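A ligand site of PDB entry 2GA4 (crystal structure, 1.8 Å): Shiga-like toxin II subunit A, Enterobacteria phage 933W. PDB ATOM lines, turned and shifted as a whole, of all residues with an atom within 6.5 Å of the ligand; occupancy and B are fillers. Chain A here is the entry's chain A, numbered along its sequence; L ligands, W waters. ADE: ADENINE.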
ATOM      1  N   ASN A  75       8.577  -4.751 -38.782  1.00  0.00           N
ATOM      2  CA  ASN A  75       8.670  -5.424 -37.490  1.00  0.00           C
ATOM      3  C   ASN A  75       8.296  -4.578 -36.341  1.00  0.00           C
ATOM      4  O   ASN A  75       8.462  -5.018 -35.195  1.00  0.00           O
ATOM      5  CB  ASN A  75      10.064  -5.943 -37.256  1.00  0.00           C
ATOM      6  CG  ASN A  75      11.108  -4.885 -37.451  1.00  0.00           C
ATOM      7  OD1 ASN A  75      10.874  -3.712 -37.224  1.00  0.00           O
ATOM      8  ND2 ASN A  75      12.310  -5.304 -37.876  1.00  0.00           N
ATOM      9  N   LEU A  76       7.849  -3.347 -36.603  1.00  0.00           N
ATOM     10  CA  LEU A  76       7.442  -2.444 -35.543  1.00  0.00           C
ATOM     11  C   LEU A  76       8.531  -2.088 -34.560  1.00  0.00           C
ATOM     12  O   LEU A  76       8.279  -1.670 -33.443  1.00  0.00           O
ATOM     13  CB  LEU A  76       6.225  -3.029 -34.808  1.00  0.00           C
ATOM     14  CG  LEU A  76       4.926  -2.980 -35.612  1.00  0.00           C
ATOM     15  CD1 LEU A  76       3.768  -3.579 -34.768  1.00  0.00           C
ATOM     16  CD2 LEU A  76       4.633  -1.477 -35.945  1.00  0.00           C
ATOM     17  N   TYR A  77       9.771  -2.220 -34.979  1.00  0.00           N
ATOM     18  CA  TYR A  77      10.848  -1.839 -34.105  1.00  0.00           C
ATOM     19  C   TYR A  77      11.034  -0.352 -34.100  1.00  0.00           C
ATOM     20  O   TYR A  77      10.911   0.285 -35.137  1.00  0.00           O
ATOM     21  CB  TYR A  77      12.143  -2.472 -34.543  1.00  0.00           C
ATOM     22  CG  TYR A  77      12.481  -3.606 -33.669  1.00  0.00           C
ATOM     23  CD1 TYR A  77      11.677  -4.744 -33.655  1.00  0.00           C
ATOM     24  CD2 TYR A  77      13.592  -3.537 -32.804  1.00  0.00           C
ATOM     25  CE1 TYR A  77      11.947  -5.786 -32.802  1.00  0.00           C
ATOM     26  CE2 TYR A  77      13.889  -4.598 -31.957  1.00  0.00           C
ATOM     27  CZ  TYR A  77      13.072  -5.710 -31.964  1.00  0.00           C
ATOM     28  OH  TYR A  77      13.372  -6.766 -31.154  1.00  0.00           O
ATOM     29  N   VAL A  78      11.324   0.208 -32.935  1.00  0.00           N
ATOM     30  CA  VAL A  78      11.615   1.637 -32.870  1.00  0.00           C
ATOM     31  C   VAL A  78      13.094   1.683 -33.242  1.00  0.00           C
ATOM     32  O   VAL A  78      13.951   1.201 -32.500  1.00  0.00           O
ATOM     33  CB  VAL A  78      11.450   2.206 -31.440  1.00  0.00           C
ATOM     34  CG1 VAL A  78      12.029   3.611 -31.380  1.00  0.00           C
ATOM     35  CG2 VAL A  78       9.938   2.229 -31.049  1.00  0.00           C
ATOM     36  N   ALA A  79      13.349   2.220 -34.422  1.00  0.00           N
ATOM     37  CA  ALA A  79      14.686   2.321 -34.983  1.00  0.00           C
ATOM     38  C   ALA A  79      15.439   3.496 -34.379  1.00  0.00           C
ATOM     39  O   ALA A  79      16.669   3.595 -34.480  1.00  0.00           O
ATOM     40  CB  ALA A  79      14.560   2.508 -36.512  1.00  0.00           C
ATOM     41  N   GLY A  80      14.708   4.398 -33.748  1.00  0.00           N
ATOM     42  CA  GLY A  80      15.353   5.547 -33.146  1.00  0.00           C
ATOM     43  C   GLY A  80      14.309   6.598 -32.877  1.00  0.00           C
ATOM     44  O   GLY A  80      13.124   6.359 -33.037  1.00  0.00           O
ATOM     45  N   PHE A  92      19.339   3.821 -33.747  1.00  0.00           N
ATOM     46  CA  PHE A  92      20.062   2.728 -33.118  1.00  0.00           C
ATOM     47  C   PHE A  92      21.028   2.104 -34.111  1.00  0.00           C
ATOM     48  O   PHE A  92      20.820   2.173 -35.323  1.00  0.00           O
ATOM     49  CB  PHE A  92      19.078   1.676 -32.613  1.00  0.00           C
ATOM     50  CG  PHE A  92      18.381   2.093 -31.372  1.00  0.00           C
ATOM     51  CD1 PHE A  92      19.103   2.282 -30.202  1.00  0.00           C
ATOM     52  CD2 PHE A  92      17.015   2.343 -31.375  1.00  0.00           C
ATOM     53  CE1 PHE A  92      18.482   2.729 -29.053  1.00  0.00           C
ATOM     54  CE2 PHE A  92      16.376   2.804 -30.218  1.00  0.00           C
ATOM     55  CZ  PHE A  92      17.097   2.984 -29.068  1.00  0.00           C
ATOM     56  N   PHE A  95      20.006  -0.239 -36.976  1.00  0.00           N
ATOM     57  CA  PHE A  95      19.035   0.260 -37.926  1.00  0.00           C
ATOM     58  C   PHE A  95      19.648   1.187 -38.951  1.00  0.00           C
ATOM     59  O   PHE A  95      18.988   2.107 -39.446  1.00  0.00           O
ATOM     60  CB  PHE A  95      17.921   0.943 -37.138  1.00  0.00           C
ATOM     61  CG  PHE A  95      16.982  -0.009 -36.546  1.00  0.00           C
ATOM     62  CD1 PHE A  95      15.993  -0.583 -37.335  1.00  0.00           C
ATOM     63  CD2 PHE A  95      17.136  -0.429 -35.237  1.00  0.00           C
ATOM     64  CE1 PHE A  95      15.165  -1.590 -36.821  1.00  0.00           C
ATOM     65  CE2 PHE A  95      16.330  -1.417 -34.707  1.00  0.00           C
ATOM     66  CZ  PHE A  95      15.339  -2.015 -35.501  1.00  0.00           C
ATOM     67  N   SER A 112      19.311  -1.374 -30.500  1.00  0.00           N
ATOM     68  CA  SER A 112      17.922  -1.317 -30.017  1.00  0.00           C
ATOM     69  C   SER A 112      17.429  -2.419 -29.087  1.00  0.00           C
ATOM     70  O   SER A 112      16.291  -2.342 -28.594  1.00  0.00           O
ATOM     71  CB  SER A 112      16.982  -1.349 -31.227  1.00  0.00           C
ATOM     72  OG  SER A 112      17.004  -2.662 -31.743  1.00  0.00           O
ATOM     73  N   SER A 113      18.249  -3.440 -28.850  1.00  0.00           N
ATOM     74  CA  SER A 113      17.772  -4.565 -28.065  1.00  0.00           C
ATOM     75  C   SER A 113      17.433  -4.254 -26.628  1.00  0.00           C
ATOM     76  O   SER A 113      17.983  -3.324 -26.018  1.00  0.00           O
ATOM     77  CB  SER A 113      18.805  -5.700 -28.082  1.00  0.00           C
ATOM     78  OG  SER A 113      19.905  -5.388 -27.236  1.00  0.00           O
ATOM     79  N   TYR A 114      16.502  -5.039 -26.089  1.00  0.00           N
ATOM     80  CA  TYR A 114      16.163  -4.877 -24.708  1.00  0.00           C
ATOM     81  C   TYR A 114      17.345  -5.277 -23.842  1.00  0.00           C
ATOM     82  O   TYR A 114      17.521  -4.724 -22.772  1.00  0.00           O
ATOM     83  CB  TYR A 114      14.991  -5.753 -24.334  1.00  0.00           C
ATOM     84  CG  TYR A 114      13.672  -5.187 -24.867  1.00  0.00           C
ATOM     85  CD1 TYR A 114      13.424  -3.815 -24.791  1.00  0.00           C
ATOM     86  CD2 TYR A 114      12.661  -6.027 -25.335  1.00  0.00           C
ATOM     87  CE1 TYR A 114      12.199  -3.297 -25.166  1.00  0.00           C
ATOM     88  CE2 TYR A 114      11.404  -5.504 -25.717  1.00  0.00           C
ATOM     89  CZ  TYR A 114      11.198  -4.136 -25.625  1.00  0.00           C
ATOM     90  OH  TYR A 114       9.990  -3.569 -25.983  1.00  0.00           O
ATOM     91  N   LEU A 117      19.289  -2.094 -23.890  1.00  0.00           N
ATOM     92  CA  LEU A 117      18.600  -0.996 -23.267  1.00  0.00           C
ATOM     93  C   LEU A 117      18.441  -1.145 -21.794  1.00  0.00           C
ATOM     94  O   LEU A 117      18.628  -0.178 -21.072  1.00  0.00           O
ATOM     95  CB  LEU A 117      17.232  -0.729 -23.922  1.00  0.00           C
ATOM     96  CG  LEU A 117      17.348  -0.191 -25.342  1.00  0.00           C
ATOM     97  CD1 LEU A 117      15.910  -0.055 -25.910  1.00  0.00           C
ATOM     98  CD2 LEU A 117      18.017   1.156 -25.379  1.00  0.00           C
ATOM     99  N   ARG A 125      12.695  -4.459 -17.524  1.00  0.00           N
ATOM    100  CA  ARG A 125      11.336  -4.247 -17.965  1.00  0.00           C
ATOM    101  C   ARG A 125      10.356  -4.930 -17.036  1.00  0.00           C
ATOM    102  O   ARG A 125       9.253  -4.430 -16.823  1.00  0.00           O
ATOM    103  CB  ARG A 125      11.111  -4.788 -19.382  1.00  0.00           C
ATOM    104  CG  ARG A 125      11.949  -4.093 -20.399  1.00  0.00           C
ATOM    105  CD  ARG A 125      11.398  -4.398 -21.773  1.00  0.00           C
ATOM    106  NE  ARG A 125      11.571  -5.800 -22.085  1.00  0.00           N
ATOM    107  CZ  ARG A 125      10.646  -6.538 -22.676  1.00  0.00           C
ATOM    108  NH1 ARG A 125       9.461  -6.005 -23.024  1.00  0.00           N
ATOM    109  NH2 ARG A 125      10.926  -7.798 -22.968  1.00  0.00           N
ATOM    110  N   VAL A 158      13.518   5.332 -23.743  1.00  0.00           N
ATOM    111  CA  VAL A 158      13.200   4.479 -24.882  1.00  0.00           C
ATOM    112  C   VAL A 158      12.491   3.229 -24.408  1.00  0.00           C
ATOM    113  O   VAL A 158      11.547   2.782 -25.049  1.00  0.00           O
ATOM    114  CB  VAL A 158      14.457   4.119 -25.714  1.00  0.00           C
ATOM    115  CG1 VAL A 158      14.133   3.020 -26.749  1.00  0.00           C
ATOM    116  CG2 VAL A 158      14.960   5.383 -26.428  1.00  0.00           C
ATOM    117  N   VAL A 162       8.972   2.579 -26.036  1.00  0.00           N
ATOM    118  CA  VAL A 162       8.808   1.411 -26.890  1.00  0.00           C
ATOM    119  C   VAL A 162       7.660   0.573 -26.342  1.00  0.00           C
ATOM    120  O   VAL A 162       6.851   0.019 -27.092  1.00  0.00           O
ATOM    121  CB  VAL A 162      10.102   0.576 -26.932  1.00  0.00           C
ATOM    122  CG1 VAL A 162       9.860  -0.810 -27.504  1.00  0.00           C
ATOM    123  CG2 VAL A 162      11.087   1.308 -27.809  1.00  0.00           C
ATOM    124  N   ALA A 166       5.276   0.665 -29.673  1.00  0.00           N
ATOM    125  CA  ALA A 166       5.436  -0.587 -30.413  1.00  0.00           C
ATOM    126  C   ALA A 166       4.862  -1.782 -29.680  1.00  0.00           C
ATOM    127  O   ALA A 166       4.179  -2.581 -30.294  1.00  0.00           O
ATOM    128  CB  ALA A 166       6.924  -0.851 -30.711  1.00  0.00           C
ATOM    129  N   GLU A 167       5.137  -1.949 -28.381  1.00  0.00           N
ATOM    130  CA  GLU A 167       4.643  -3.186 -27.757  1.00  0.00           C
ATOM    131  C   GLU A 167       3.130  -3.159 -27.637  1.00  0.00           C
ATOM    132  O   GLU A 167       2.474  -4.179 -27.787  1.00  0.00           O
ATOM    133  CB  GLU A 167       5.309  -3.433 -26.390  1.00  0.00           C
ATOM    134  CG  GLU A 167       6.819  -3.615 -26.486  1.00  0.00           C
ATOM    135  CD  GLU A 167       7.279  -4.881 -27.244  1.00  0.00           C
ATOM    136  OE1 GLU A 167       6.485  -5.593 -27.916  1.00  0.00           O
ATOM    137  OE2 GLU A 167       8.503  -5.151 -27.193  1.00  0.00           O
ATOM    138  N   ARG A 170       1.594  -4.077 -30.917  1.00  0.00           N
ATOM    139  CA  ARG A 170       1.613  -5.531 -31.099  1.00  0.00           C
ATOM    140  C   ARG A 170       0.626  -6.261 -30.208  1.00  0.00           C
ATOM    141  O   ARG A 170      -0.059  -7.178 -30.643  1.00  0.00           O
ATOM    142  CB  ARG A 170       2.966  -6.071 -30.738  1.00  0.00           C
ATOM    143  CG  ARG A 170       4.055  -5.624 -31.666  1.00  0.00           C
ATOM    144  CD  ARG A 170       5.411  -6.119 -31.086  1.00  0.00           C
ATOM    145  NE  ARG A 170       6.493  -5.736 -31.976  1.00  0.00           N
ATOM    146  CZ  ARG A 170       7.602  -5.124 -31.570  1.00  0.00           C
ATOM    147  NH1 ARG A 170       7.753  -4.819 -30.297  1.00  0.00           N
ATOM    148  NH2 ARG A 170       8.582  -4.867 -32.423  1.00  0.00           N
ATOM    149  N   THR A 199       6.029  -9.991 -25.090  1.00  0.00           N
ATOM    150  CA  THR A 199       6.894  -9.287 -26.009  1.00  0.00           C
ATOM    151  C   THR A 199       8.060 -10.151 -26.487  1.00  0.00           C
ATOM    152  O   THR A 199       8.530  -9.993 -27.594  1.00  0.00           O
ATOM    153  CB  THR A 199       7.446  -7.967 -25.409  1.00  0.00           C
ATOM    154  OG1 THR A 199       8.345  -8.247 -24.297  1.00  0.00           O
ATOM    155  CG2 THR A 199       6.248  -7.071 -24.920  1.00  0.00           C
HETATM  156  N9  ADE L   1      11.982  -4.769 -28.784  1.00  0.00           N
HETATM  157  C8  ADE L   1      13.269  -4.599 -28.374  1.00  0.00           C
HETATM  158  N7  ADE L   1      13.824  -3.426 -28.691  1.00  0.00           N
HETATM  159  C5  ADE L   1      12.782  -2.794 -29.391  1.00  0.00           C
HETATM  160  C6  ADE L   1      12.675  -1.534 -30.028  1.00  0.00           C
HETATM  161  N6  ADE L   1      13.722  -0.684 -30.014  1.00  0.00           N
HETATM  162  N1  ADE L   1      11.469  -1.217 -30.637  1.00  0.00           N
HETATM  163  C2  ADE L   1      10.408  -2.101 -30.641  1.00  0.00           C
HETATM  164  N3  ADE L   1      10.393  -3.326 -30.063  1.00  0.00           N
HETATM  165  C4  ADE L   1      11.640  -3.620 -29.449  1.00  0.00           C
HETATM  166  O   HOH W   1      10.170  -6.781 -28.553  1.00  0.00           O
HETATM  167  O   HOH W   2      15.379  -7.020 -27.755  1.00  0.00           O
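O of Ser 112 is in hydrogen-bond range of N6 of the ligand. The guanidinium group (NH1) of Arg 170 sits at hydrogen-bond distance from a nitrogen (N3) of the ligand. The side-chain hydroxyl of Tyr 77 sits at hydrogen-bond distance from a nitrogen (N9) of the ligand, 3.4 Å away. A nitrogen (N1) of the ligand sits at hydrogen-bond distance from the backbone NH of Val 78 (2.7 Å). A nitrogen (N6) of the ligand is in hydrogen-bond range of the backbone carbonyl oxygen (O) of Val 78 (3.1 Å).
The backbone carbonyl oxygen (O) of Val 162 is in hydrogen-bond range of the backbone NH (N) of Glu 167 (2.9 Å). The guanidinium group (NH1) of Arg 170 lies within salt-bridge range of the side-chain carboxylate (OE1) of Glu 167, 2.8 Å away. The side-chain hydroxyl of Tyr 114 is in hydrogen-bond range of the side-chain carboxylate of Glu 167 (2.5 Å). The guanidinium group (NH2) of Arg 170 is in hydrogen-bond range of the backbone carbonyl oxygen (O) of Asn 75, at 2.8 Å. OD1 of Asn 75 is in hydrogen-bond range of N of Tyr 77, at 2.9 Å. O of Leu 76 is in hydrogen-bond range of NH2 of Arg 170, 3.4 Å away.
Leu 76 touches the ligand. CE2 of Tyr 114 touches N9 of the ligand (3.2 Å). CG1 of Val 162 touches C2 of the ligand, 3.4 Å away. Ala 166 touches the ligand. Glu 167 touches the ligand. Hydrophobic or aromatic side chains that line the ligand: Tyr 77, Val 78, Tyr 114, Val 162 and Ala 166. Within 4 Å of the ligand: Leu 76, Tyr 77, Val 78, Ser 112, Tyr 114, Val 162, Ala 166, Glu 167 and Arg 170. Along chain A the residues within 4 Å of the ligand span positions 76 to 170. The nearest printed residue that does not touch the ligand is Ser 113 (4.2 Å).
Water W1 lies within hydrogen-bond range of the side-chain carboxylate of Glu 167 (2.7 Å) and a nitrogen (N9) of the ligand (2.7 Å).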
